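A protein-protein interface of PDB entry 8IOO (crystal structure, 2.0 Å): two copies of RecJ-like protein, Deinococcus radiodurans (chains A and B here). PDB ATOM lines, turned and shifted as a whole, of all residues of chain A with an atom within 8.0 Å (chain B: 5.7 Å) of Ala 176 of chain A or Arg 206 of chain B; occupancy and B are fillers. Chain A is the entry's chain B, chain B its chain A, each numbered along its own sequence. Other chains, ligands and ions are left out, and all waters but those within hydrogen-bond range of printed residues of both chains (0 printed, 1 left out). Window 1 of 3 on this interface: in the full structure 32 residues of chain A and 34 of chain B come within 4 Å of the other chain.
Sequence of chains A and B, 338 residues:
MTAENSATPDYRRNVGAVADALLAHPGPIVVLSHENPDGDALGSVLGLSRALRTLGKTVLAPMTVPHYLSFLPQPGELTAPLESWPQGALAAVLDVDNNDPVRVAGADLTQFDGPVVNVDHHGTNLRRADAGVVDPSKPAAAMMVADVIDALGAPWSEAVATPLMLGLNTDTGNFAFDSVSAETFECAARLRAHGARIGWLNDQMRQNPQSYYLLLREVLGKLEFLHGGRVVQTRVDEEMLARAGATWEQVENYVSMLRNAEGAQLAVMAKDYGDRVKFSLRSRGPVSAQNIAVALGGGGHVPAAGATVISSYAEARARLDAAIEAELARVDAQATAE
The side-chain hydroxyl (OG1) of Thr 172 of chain A is in hydrogen-bond range of the backbone NH (N) of Phe 175 of chain A, 3.1 Å away. The backbone carbonyl oxygen (O) of Ser 256 of chain A sits at hydrogen-bond distance from the side-chain amide nitrogen (ND2) of Asn 260 of chain A, 3.3 Å away. The backbone NH (N) of Asn 174 of chain A sits at hydrogen-bond distance from the backbone carbonyl oxygen (O) of Asn 169 of chain A (2.9 Å). The side-chain amide oxygen of Asn 202 of chain B lies within hydrogen-bond range of the guanidinium group of Arg 206 of chain B (2.7 Å). The backbone carbonyl oxygen of Ile 198 of chain B is in hydrogen-bond range of the side-chain amide nitrogen of Asn 202 of chain B (3.2 Å). The backbone carbonyl oxygen (O) of Thr 172 of chain A is in hydrogen-bond range of the backbone NH (N) of Phe 177 of chain A.
Among the printed residues, no Asp or Glu carboxylate lies within 4 Å of a Lys or Arg side-chain nitrogen of the other chain.
The backbone carbonyl oxygen (O) of Arg 206 of chain B lies close to the backbone carbonyl oxygen (O) of Asn 260 of chain A (2.8 Å). The side-chain amide nitrogen (ND2) of Asn 174 of chain B is in hydrogen-bond range of the backbone carbonyl oxygen (O) of Asn 174 of chain A, at 3.5 Å. The side-chain carboxylate (OE2) of Glu 262 of chain A lies close to the backbone carbonyl oxygen (O) of Gln 207 of chain B (3.3 Å). The backbone NH (N) of Asn 208 of chain B lies within hydrogen-bond range of the backbone carbonyl oxygen (O) of Asn 260 of chain A, at 3.0 Å. The backbone carbonyl oxygen (O) of Asn 208 of chain B lies within hydrogen-bond range of the backbone NH (N) of Glu 262 of chain A, 3.1 Å away.
Asn 174 of chain B touches its own counterpart, Asn 174 of chain A. Position printed for both chains: 174. Of the 15 pairs that touch across the chains among the printed residues, 1 has its exchanged pair printed and touching as well.
Ala 176 of chain A touches just these residues of chain B: Ile 198 (3.7 Å), Gly 199 (3.7 Å), Asn 202 (3.2 Å) and Arg 206 (3.6 Å). Arg 206 of chain B touches just these residues of chain A: Ala 176 and Asn 260. Of the printed residues of chain A, Asn 174 of chain B touches Asn 174. Of the printed residues of chain A, Asn 208 of chain B touches Asn 260, Ala 261 and Glu 262. Of the printed residues of chain B, Arg 284 of chain A touches Gln 207. The nearest residue of chain B that does not touch Ala 176 of chain A is Asn 174 of chain B (4.6 Å).
O of Phe 175 of chain A touches CD1 of Ile 198 of chain B, at 3.1 Å. O of Phe 175 of chain A touches ND2 of Asn 202 of chain B, 3.9 Å away. Ile 198 of chain B touches Ala 176 of chain A. Gly 199 of chain B touches Ala 176 of chain A (CA to O, 3.7 Å). Asn 202 of chain B touches Ala 176 of chain A (ND2 to CA, 3.2 Å). Arg 206 of chain B touches Ala 176 of chain A. Phe 177 of chain A touches Ile 198 of chain B. O of Asn 260 of chain A touches CA of Gln 207 of chain B, 3.5 Å away. Ala 261 of chain A touches Asn 208 of chain B (CA to O, 3.6 Å). Arg 284 of chain A touches Gln 207 of chain B.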
ATOM      1  N   LEU A 168       5.774 -24.112 -18.385  1.00  0.00           N
ATOM      2  CA  LEU A 168       6.689 -23.800 -17.296  1.00  0.00           C
ATOM      3  C   LEU A 168       7.169 -22.357 -17.390  1.00  0.00           C
ATOM      4  O   LEU A 168       7.170 -21.625 -16.388  1.00  0.00           O
ATOM      5  CB  LEU A 168       7.854 -24.798 -17.329  1.00  0.00           C
ATOM      6  CG  LEU A 168       8.762 -24.895 -16.111  1.00  0.00           C
ATOM      7  CD1 LEU A 168       7.920 -25.197 -14.887  1.00  0.00           C
ATOM      8  CD2 LEU A 168       9.846 -25.966 -16.319  1.00  0.00           C
ATOM      9  N   ASN A 169       7.522 -21.924 -18.606  1.00  0.00           N
ATOM     10  CA  ASN A 169       7.939 -20.550 -18.885  1.00  0.00           C
ATOM     11  C   ASN A 169       6.859 -19.559 -18.465  1.00  0.00           C
ATOM     12  O   ASN A 169       7.066 -18.721 -17.582  1.00  0.00           O
ATOM     13  CB  ASN A 169       8.192 -20.366 -20.385  1.00  0.00           C
ATOM     14  CG  ASN A 169       9.540 -20.854 -20.829  1.00  0.00           C
ATOM     15  OD1 ASN A 169      10.349 -21.327 -20.036  1.00  0.00           O
ATOM     16  ND2 ASN A 169       9.800 -20.717 -22.120  1.00  0.00           N
ATOM     17  N   ASP A 171       4.000 -19.666 -16.881  1.00  0.00           N
ATOM     18  CA  ASP A 171       3.442 -19.665 -15.536  1.00  0.00           C
ATOM     19  C   ASP A 171       4.442 -19.179 -14.478  1.00  0.00           C
ATOM     20  O   ASP A 171       4.016 -18.802 -13.388  1.00  0.00           O
ATOM     21  CB  ASP A 171       2.927 -21.058 -15.146  1.00  0.00           C
ATOM     22  CG  ASP A 171       1.376 -21.147 -15.075  1.00  0.00           C
ATOM     23  OD1 ASP A 171       0.649 -20.356 -15.714  1.00  0.00           O
ATOM     24  OD2 ASP A 171       0.898 -21.986 -14.296  1.00  0.00           O
ATOM     25  N   THR A 172       5.753 -19.187 -14.761  1.00  0.00           N
ATOM     26  CA  THR A 172       6.765 -18.636 -13.856  1.00  0.00           C
ATOM     27  C   THR A 172       7.330 -17.300 -14.323  1.00  0.00           C
ATOM     28  O   THR A 172       8.331 -16.833 -13.756  1.00  0.00           O
ATOM     29  CB  THR A 172       7.940 -19.614 -13.693  1.00  0.00           C
ATOM     30  OG1 THR A 172       8.554 -19.850 -14.967  1.00  0.00           O
ATOM     31  CG2 THR A 172       7.477 -20.940 -13.149  1.00  0.00           C
ATOM     32  N   GLY A 173       6.723 -16.682 -15.334  1.00  0.00           N
ATOM     33  CA  GLY A 173       7.286 -15.505 -15.985  1.00  0.00           C
ATOM     34  C   GLY A 173       8.750 -15.625 -16.373  1.00  0.00           C
ATOM     35  O   GLY A 173       9.549 -14.744 -16.036  1.00  0.00           O
ATOM     36  N   ASN A 174       9.118 -16.696 -17.086  1.00  0.00           N
ATOM     37  CA  ASN A 174      10.518 -16.955 -17.449  1.00  0.00           C
ATOM     38  C   ASN A 174      11.403 -17.092 -16.219  1.00  0.00           C
ATOM     39  O   ASN A 174      12.510 -16.555 -16.174  1.00  0.00           O
ATOM     40  CB  ASN A 174      11.081 -15.887 -18.397  1.00  0.00           C
ATOM     41  CG  ASN A 174      10.764 -16.185 -19.853  1.00  0.00           C
ATOM     42  OD1 ASN A 174      11.506 -16.899 -20.534  1.00  0.00           O
ATOM     43  ND2 ASN A 174       9.611 -15.704 -20.317  1.00  0.00           N
ATOM     44  N   PHE A 175      10.917 -17.844 -15.239  1.00  0.00           N
ATOM     45  CA  PHE A 175      11.676 -18.199 -14.042  1.00  0.00           C
ATOM     46  C   PHE A 175      12.017 -16.959 -13.208  1.00  0.00           C
ATOM     47  O   PHE A 175      13.058 -16.915 -12.558  1.00  0.00           O
ATOM     48  CB  PHE A 175      12.941 -18.981 -14.409  1.00  0.00           C
ATOM     49  CG  PHE A 175      12.648 -20.215 -15.208  1.00  0.00           C
ATOM     50  CD1 PHE A 175      12.306 -21.396 -14.583  1.00  0.00           C
ATOM     51  CD2 PHE A 175      12.692 -20.177 -16.595  1.00  0.00           C
ATOM     52  CE1 PHE A 175      11.999 -22.519 -15.331  1.00  0.00           C
ATOM     53  CE2 PHE A 175      12.407 -21.281 -17.340  1.00  0.00           C
ATOM     54  CZ  PHE A 175      12.055 -22.459 -16.714  1.00  0.00           C
ATOM     55  N   ALA A 176      11.132 -15.955 -13.234  1.00  0.00           N
ATOM     56  CA  ALA A 176      11.329 -14.701 -12.506  1.00  0.00           C
ATOM     57  C   ALA A 176      10.558 -14.608 -11.191  1.00  0.00           C
ATOM     58  O   ALA A 176      11.004 -13.905 -10.284  1.00  0.00           O
ATOM     59  CB  ALA A 176      10.917 -13.502 -13.379  1.00  0.00           C
ATOM     60  N   PHE A 177       9.408 -15.273 -11.076  1.00  0.00           N
ATOM     61  CA  PHE A 177       8.595 -15.188  -9.864  1.00  0.00           C
ATOM     62  C   PHE A 177       9.259 -15.920  -8.702  1.00  0.00           C
ATOM     63  O   PHE A 177      10.059 -16.843  -8.890  1.00  0.00           O
ATOM     64  CB  PHE A 177       7.201 -15.776 -10.092  1.00  0.00           C
ATOM     65  CG  PHE A 177       6.444 -15.183 -11.252  1.00  0.00           C
ATOM     66  CD1 PHE A 177       6.798 -13.953 -11.789  1.00  0.00           C
ATOM     67  CD2 PHE A 177       5.379 -15.880 -11.825  1.00  0.00           C
ATOM     68  CE1 PHE A 177       6.092 -13.409 -12.855  1.00  0.00           C
ATOM     69  CE2 PHE A 177       4.669 -15.343 -12.900  1.00  0.00           C
ATOM     70  CZ  PHE A 177       5.028 -14.103 -13.414  1.00  0.00           C
ATOM     71  N   ASP A 178       8.891 -15.518  -7.480  1.00  0.00           N
ATOM     72  CA  ASP A 178       9.421 -16.165  -6.284  1.00  0.00           C
ATOM     73  C   ASP A 178       8.839 -17.560  -6.061  1.00  0.00           C
ATOM     74  O   ASP A 178       9.299 -18.272  -5.160  1.00  0.00           O
ATOM     75  CB  ASP A 178       9.160 -15.323  -5.037  1.00  0.00           C
ATOM     76  CG  ASP A 178       7.705 -14.921  -4.899  1.00  0.00           C
ATOM     77  OD1 ASP A 178       6.836 -15.821  -4.885  1.00  0.00           O
ATOM     78  OD2 ASP A 178       7.435 -13.708  -4.802  1.00  0.00           O
ATOM     79  N   SER A 179       7.824 -17.947  -6.843  1.00  0.00           N
ATOM     80  CA  SER A 179       7.338 -19.325  -6.828  1.00  0.00           C
ATOM     81  C   SER A 179       8.351 -20.313  -7.412  1.00  0.00           C
ATOM     82  O   SER A 179       8.220 -21.524  -7.204  1.00  0.00           O
ATOM     83  CB  SER A 179       6.003 -19.424  -7.589  1.00  0.00           C
ATOM     84  OG  SER A 179       6.159 -18.970  -8.925  1.00  0.00           O
ATOM     85  N   VAL A 180       9.373 -19.826  -8.112  1.00  0.00           N
ATOM     86  CA  VAL A 180      10.381 -20.700  -8.709  1.00  0.00           C
ATOM     87  C   VAL A 180      11.239 -21.310  -7.602  1.00  0.00           C
ATOM     88  O   VAL A 180      11.968 -20.602  -6.893  1.00  0.00           O
ATOM     89  CB  VAL A 180      11.228 -19.906  -9.711  1.00  0.00           C
ATOM     90  CG1 VAL A 180      12.346 -20.794 -10.335  1.00  0.00           C
ATOM     91  CG2 VAL A 180      10.318 -19.287 -10.764  1.00  0.00           C
ATOM     92  N   PHE A 185      13.572 -25.627 -11.447  1.00  0.00           N
ATOM     93  CA  PHE A 185      14.691 -25.586 -12.378  1.00  0.00           C
ATOM     94  C   PHE A 185      15.087 -26.995 -12.784  1.00  0.00           C
ATOM     95  O   PHE A 185      15.453 -27.227 -13.934  1.00  0.00           O
ATOM     96  CB  PHE A 185      15.882 -24.855 -11.735  1.00  0.00           C
ATOM     97  CG  PHE A 185      15.797 -23.337 -11.816  1.00  0.00           C
ATOM     98  CD1 PHE A 185      15.523 -22.678 -12.996  1.00  0.00           C
ATOM     99  CD2 PHE A 185      15.944 -22.576 -10.665  1.00  0.00           C
ATOM    100  CE1 PHE A 185      15.433 -21.281 -13.032  1.00  0.00           C
ATOM    101  CE2 PHE A 185      15.864 -21.191 -10.700  1.00  0.00           C
ATOM    102  CZ  PHE A 185      15.610 -20.542 -11.889  1.00  0.00           C
ATOM    103  N   SER A 256       1.378  -4.935 -15.869  1.00  0.00           N
ATOM    104  CA  SER A 256       2.612  -5.551 -15.385  1.00  0.00           C
ATOM    105  C   SER A 256       3.818  -4.654 -15.621  1.00  0.00           C
ATOM    106  O   SER A 256       4.683  -4.517 -14.748  1.00  0.00           O
ATOM    107  CB  SER A 256       2.814  -6.912 -16.059  1.00  0.00           C
ATOM    108  OG  SER A 256       2.791  -6.777 -17.469  1.00  0.00           O
ATOM    109  N   MET A 257       3.847  -4.004 -16.788  1.00  0.00           N
ATOM    110  CA  MET A 257       4.969  -3.099 -17.158  1.00  0.00           C
ATOM    111  C   MET A 257       4.937  -1.832 -16.299  1.00  0.00           C
ATOM    112  O   MET A 257       6.006  -1.252 -16.053  1.00  0.00           O
ATOM    113  CB  MET A 257       4.853  -2.711 -18.633  1.00  0.00           C
ATOM    114  CG  MET A 257       5.166  -1.259 -18.917  1.00  0.00           C
ATOM    115  SD  MET A 257       4.744  -0.828 -20.613  1.00  0.00           S
ATOM    116  CE  MET A 257       4.596  -2.462 -21.333  1.00  0.00           C
ATOM    117  N   LEU A 258       3.751  -1.421 -15.864  1.00  0.00           N
ATOM    118  CA  LEU A 258       3.651  -0.174 -15.077  1.00  0.00           C
ATOM    119  C   LEU A 258       4.032  -0.466 -13.627  1.00  0.00           C
ATOM    120  O   LEU A 258       4.505   0.463 -12.961  1.00  0.00           O
ATOM    121  CB  LEU A 258       2.225   0.371 -15.179  1.00  0.00           C
ATOM    122  CG  LEU A 258       2.004   1.428 -16.258  1.00  0.00           C
ATOM    123  CD1 LEU A 258       0.838   2.329 -15.891  1.00  0.00           C
ATOM    124  CD2 LEU A 258       3.263   2.253 -16.467  1.00  0.00           C
ATOM    125  N   ARG A 259       3.821  -1.701 -13.155  1.00  0.00           N
ATOM    126  CA  ARG A 259       4.293  -1.988 -11.777  1.00  0.00           C
ATOM    127  C   ARG A 259       5.812  -1.813 -11.746  1.00  0.00           C
ATOM    128  O   ARG A 259       6.345  -1.476 -10.677  1.00  0.00           O
ATOM    129  CB  ARG A 259       3.916  -3.427 -11.421  1.00  0.00           C
ATOM    130  CG  ARG A 259       4.067  -3.775  -9.950  1.00  0.00           C
ATOM    131  CD  ARG A 259       4.708  -5.139  -9.792  1.00  0.00           C
ATOM    132  NE  ARG A 259       3.722  -6.207  -9.852  1.00  0.00           N
ATOM    133  CZ  ARG A 259       3.629  -7.096 -10.833  1.00  0.00           C
ATOM    134  NH1 ARG A 259       4.466  -7.050 -11.856  1.00  0.00           N
ATOM    135  NH2 ARG A 259       2.696  -8.029 -10.789  1.00  0.00           N
ATOM    136  N   ASN A 260       6.464  -1.935 -12.901  1.00  0.00           N
ATOM    137  CA  ASN A 260       7.949  -1.924 -12.966  1.00  0.00           C
ATOM    138  C   ASN A 260       8.546  -0.514 -12.837  1.00  0.00           C
ATOM    139  O   ASN A 260       9.755  -0.398 -13.021  1.00  0.00           O
ATOM    140  CB  ASN A 260       8.396  -2.625 -14.253  1.00  0.00           C
ATOM    141  CG  ASN A 260       8.009  -4.086 -14.310  1.00  0.00           C
ATOM    142  OD1 ASN A 260       7.853  -4.736 -13.281  1.00  0.00           O
ATOM    143  ND2 ASN A 260       7.864  -4.615 -15.512  1.00  0.00           N
ATOM    144  N   ALA A 261       7.755   0.498 -12.499  1.00  0.00           N
ATOM    145  CA  ALA A 261       8.291   1.878 -12.476  1.00  0.00           C
ATOM    146  C   ALA A 261       9.054   2.149 -11.180  1.00  0.00           C
ATOM    147  O   ALA A 261       8.701   1.563 -10.149  1.00  0.00           O
ATOM    148  CB  ALA A 261       7.183   2.873 -12.691  1.00  0.00           C
ATOM    149  N   GLU A 262      10.036   3.043 -11.231  1.00  0.00           N
ATOM    150  CA  GLU A 262      10.907   3.296 -10.059  1.00  0.00           C
ATOM    151  C   GLU A 262      10.318   4.339  -9.115  1.00  0.00           C
ATOM    152  O   GLU A 262       9.366   5.016  -9.525  1.00  0.00           O
ATOM    153  CB  GLU A 262      12.235   3.881 -10.534  1.00  0.00           C
ATOM    154  CG  GLU A 262      13.423   2.944 -10.420  1.00  0.00           C
ATOM    155  CD  GLU A 262      14.736   3.537 -10.905  1.00  0.00           C
ATOM    156  OE1 GLU A 262      14.906   4.766 -10.793  1.00  0.00           O
ATOM    157  OE2 GLU A 262      15.587   2.771 -11.396  1.00  0.00           O
ATOM    158  N   ARG A 284       3.720  -2.626  -5.191  1.00  0.00           N
ATOM    159  CA  ARG A 284       5.008  -3.201  -4.819  1.00  0.00           C
ATOM    160  C   ARG A 284       5.538  -2.449  -3.602  1.00  0.00           C
ATOM    161  O   ARG A 284       5.371  -1.231  -3.504  1.00  0.00           O
ATOM    162  CB  ARG A 284       6.005  -3.120  -5.993  1.00  0.00           C
ATOM    163  CG  ARG A 284       7.149  -4.148  -6.008  1.00  0.00           C
ATOM    164  CD  ARG A 284       8.229  -3.731  -7.034  1.00  0.00           C
ATOM    165  NE  ARG A 284       8.693  -2.354  -6.888  1.00  0.00           N
ATOM    166  CZ  ARG A 284       9.240  -1.843  -5.793  1.00  0.00           C
ATOM    167  NH1 ARG A 284       9.583  -2.605  -4.762  1.00  0.00           N
ATOM    168  NH2 ARG A 284       9.476  -0.536  -5.741  1.00  0.00           N
ATOM    169  N   ASN B 174      17.249 -14.699 -19.271  1.00  0.00           N
ATOM    170  CA  ASN B 174      16.251 -15.379 -18.449  1.00  0.00           C
ATOM    171  C   ASN B 174      15.950 -16.780 -18.967  1.00  0.00           C
ATOM    172  O   ASN B 174      14.788 -17.159 -19.137  1.00  0.00           O
ATOM    173  CB  ASN B 174      14.957 -14.574 -18.347  1.00  0.00           C
ATOM    174  CG  ASN B 174      15.051 -13.482 -17.344  1.00  0.00           C
ATOM    175  OD1 ASN B 174      15.620 -12.424 -17.609  1.00  0.00           O
ATOM    176  ND2 ASN B 174      14.527 -13.742 -16.149  1.00  0.00           N
ATOM    177  N   ILE B 198      15.703 -15.022  -6.272  1.00  0.00           N
ATOM    178  CA  ILE B 198      15.257 -14.946  -7.657  1.00  0.00           C
ATOM    179  C   ILE B 198      14.222 -13.819  -7.828  1.00  0.00           C
ATOM    180  O   ILE B 198      14.283 -13.029  -8.782  1.00  0.00           O
ATOM    181  CB  ILE B 198      14.703 -16.322  -8.058  1.00  0.00           C
ATOM    182  CG1 ILE B 198      14.173 -16.331  -9.469  1.00  0.00           C
ATOM    183  CG2 ILE B 198      13.552 -16.677  -7.179  1.00  0.00           C
ATOM    184  CD1 ILE B 198      15.289 -16.662 -10.356  1.00  0.00           C
ATOM    185  N   GLY B 199      13.291 -13.687  -6.879  1.00  0.00           N
ATOM    186  CA  GLY B 199      12.263 -12.663  -6.989  1.00  0.00           C
ATOM    187  C   GLY B 199      12.812 -11.251  -6.899  1.00  0.00           C
ATOM    188  O   GLY B 199      12.547 -10.408  -7.767  1.00  0.00           O
ATOM    189  N   LEU B 201      15.919 -10.291  -7.474  1.00  0.00           N
ATOM    190  CA  LEU B 201      16.711 -10.014  -8.675  1.00  0.00           C
ATOM    191  C   LEU B 201      15.846  -9.499  -9.818  1.00  0.00           C
ATOM    192  O   LEU B 201      16.156  -8.469 -10.434  1.00  0.00           O
ATOM    193  CB  LEU B 201      17.500 -11.261  -9.119  1.00  0.00           C
ATOM    194  CG  LEU B 201      18.650 -11.779  -8.249  1.00  0.00           C
ATOM    195  CD1 LEU B 201      19.304 -13.066  -8.838  1.00  0.00           C
ATOM    196  CD2 LEU B 201      19.692 -10.646  -8.126  1.00  0.00           C
ATOM    197  N   ASN B 202      14.722 -10.172 -10.092  1.00  0.00           N
ATOM    198  CA  ASN B 202      13.892  -9.762 -11.232  1.00  0.00           C
ATOM    199  C   ASN B 202      13.113  -8.479 -10.948  1.00  0.00           C
ATOM    200  O   ASN B 202      12.963  -7.647 -11.852  1.00  0.00           O
ATOM    201  CB  ASN B 202      13.004 -10.934 -11.661  1.00  0.00           C
ATOM    202  CG  ASN B 202      13.786 -11.962 -12.516  1.00  0.00           C
ATOM    203  OD1 ASN B 202      14.248 -11.673 -13.620  1.00  0.00           O
ATOM    204  ND2 ASN B 202      14.027 -13.140 -11.938  1.00  0.00           N
ATOM    205  N   ASP B 203      12.686  -8.251  -9.699  1.00  0.00           N
ATOM    206  CA  ASP B 203      12.257  -6.897  -9.318  1.00  0.00           C
ATOM    207  C   ASP B 203      13.286  -5.843  -9.702  1.00  0.00           C
ATOM    208  O   ASP B 203      12.978  -4.889 -10.427  1.00  0.00           O
ATOM    209  CB  ASP B 203      11.997  -6.757  -7.821  1.00  0.00           C
ATOM    210  CG  ASP B 203      10.694  -7.347  -7.385  1.00  0.00           C
ATOM    211  OD1 ASP B 203       9.826  -7.628  -8.239  1.00  0.00           O
ATOM    212  OD2 ASP B 203      10.527  -7.464  -6.161  1.00  0.00           O
ATOM    213  N   GLN B 204      14.521  -5.987  -9.193  1.00  0.00           N
ATOM    214  CA  GLN B 204      15.537  -4.952  -9.392  1.00  0.00           C
ATOM    215  C   GLN B 204      15.880  -4.759 -10.860  1.00  0.00           C
ATOM    216  O   GLN B 204      16.232  -3.641 -11.262  1.00  0.00           O
ATOM    217  CB  GLN B 204      16.789  -5.300  -8.582  1.00  0.00           C
ATOM    218  CG  GLN B 204      16.560  -5.354  -7.098  1.00  0.00           C
ATOM    219  CD  GLN B 204      16.204  -3.988  -6.502  1.00  0.00           C
ATOM    220  OE1 GLN B 204      16.629  -2.941  -6.999  1.00  0.00           O
ATOM    221  NE2 GLN B 204      15.360  -4.002  -5.480  1.00  0.00           N
ATOM    222  N   MET B 205      15.790  -5.827 -11.663  1.00  0.00           N
ATOM    223  CA  MET B 205      16.131  -5.745 -13.078  1.00  0.00           C
ATOM    224  C   MET B 205      15.036  -5.051 -13.878  1.00  0.00           C
ATOM    225  O   MET B 205      15.301  -4.547 -14.975  1.00  0.00           O
ATOM    226  CB  MET B 205      16.365  -7.151 -13.635  1.00  0.00           C
ATOM    227  CG  MET B 205      17.702  -7.745 -13.221  1.00  0.00           C
ATOM    228  SD  MET B 205      19.128  -6.712 -13.594  1.00  0.00           S
ATOM    229  CE  MET B 205      19.320  -7.140 -15.320  1.00  0.00           C
ATOM    230  N   ARG B 206      13.819  -5.017 -13.344  1.00  0.00           N
ATOM    231  CA  ARG B 206      12.705  -4.338 -13.988  1.00  0.00           C
ATOM    232  C   ARG B 206      12.413  -3.072 -13.191  1.00  0.00           C
ATOM    233  O   ARG B 206      11.242  -2.788 -12.897  1.00  0.00           O
ATOM    234  CB  ARG B 206      11.488  -5.271 -14.069  1.00  0.00           C
ATOM    235  CG  ARG B 206      11.726  -6.492 -14.959  1.00  0.00           C
ATOM    236  CD  ARG B 206      10.868  -7.644 -14.490  1.00  0.00           C
ATOM    237  NE  ARG B 206      11.621  -8.894 -14.466  1.00  0.00           N
ATOM    238  CZ  ARG B 206      11.630  -9.785 -15.444  1.00  0.00           C
ATOM    239  NH1 ARG B 206      10.920  -9.609 -16.545  1.00  0.00           N
ATOM    240  NH2 ARG B 206      12.356 -10.890 -15.305  1.00  0.00           N
ATOM    241  N   GLN B 207      13.424  -2.259 -12.939  1.00  0.00           N
ATOM    242  CA  GLN B 207      13.161  -0.957 -12.287  1.00  0.00           C
ATOM    243  C   GLN B 207      13.430   0.127 -13.336  1.00  0.00           C
ATOM    244  O   GLN B 207      14.601   0.479 -13.545  1.00  0.00           O
ATOM    245  CB  GLN B 207      14.003  -0.828 -11.020  1.00  0.00           C
ATOM    246  CG  GLN B 207      13.490  -1.660  -9.859  1.00  0.00           C
ATOM    247  CD  GLN B 207      12.185  -1.126  -9.327  1.00  0.00           C
ATOM    248  OE1 GLN B 207      12.150  -0.144  -8.592  1.00  0.00           O
ATOM    249  NE2 GLN B 207      11.094  -1.771  -9.703  1.00  0.00           N
ATOM    250  N   ASN B 208      12.371   0.597 -13.993  1.00  0.00           N
ATOM    251  CA  ASN B 208      12.474   1.499 -15.167  1.00  0.00           C
ATOM    252  C   ASN B 208      12.249   2.942 -14.710  1.00  0.00           C
ATOM    253  O   ASN B 208      11.245   3.197 -14.027  1.00  0.00           O
ATOM    254  CB  ASN B 208      11.469   1.116 -16.251  1.00  0.00           C
ATOM    255  CG  ASN B 208      11.766  -0.210 -16.912  1.00  0.00           C
ATOM    256  OD1 ASN B 208      12.897  -0.473 -17.309  1.00  0.00           O
ATOM    257  ND2 ASN B 208      10.750  -1.045 -17.042  1.00  0.00           N
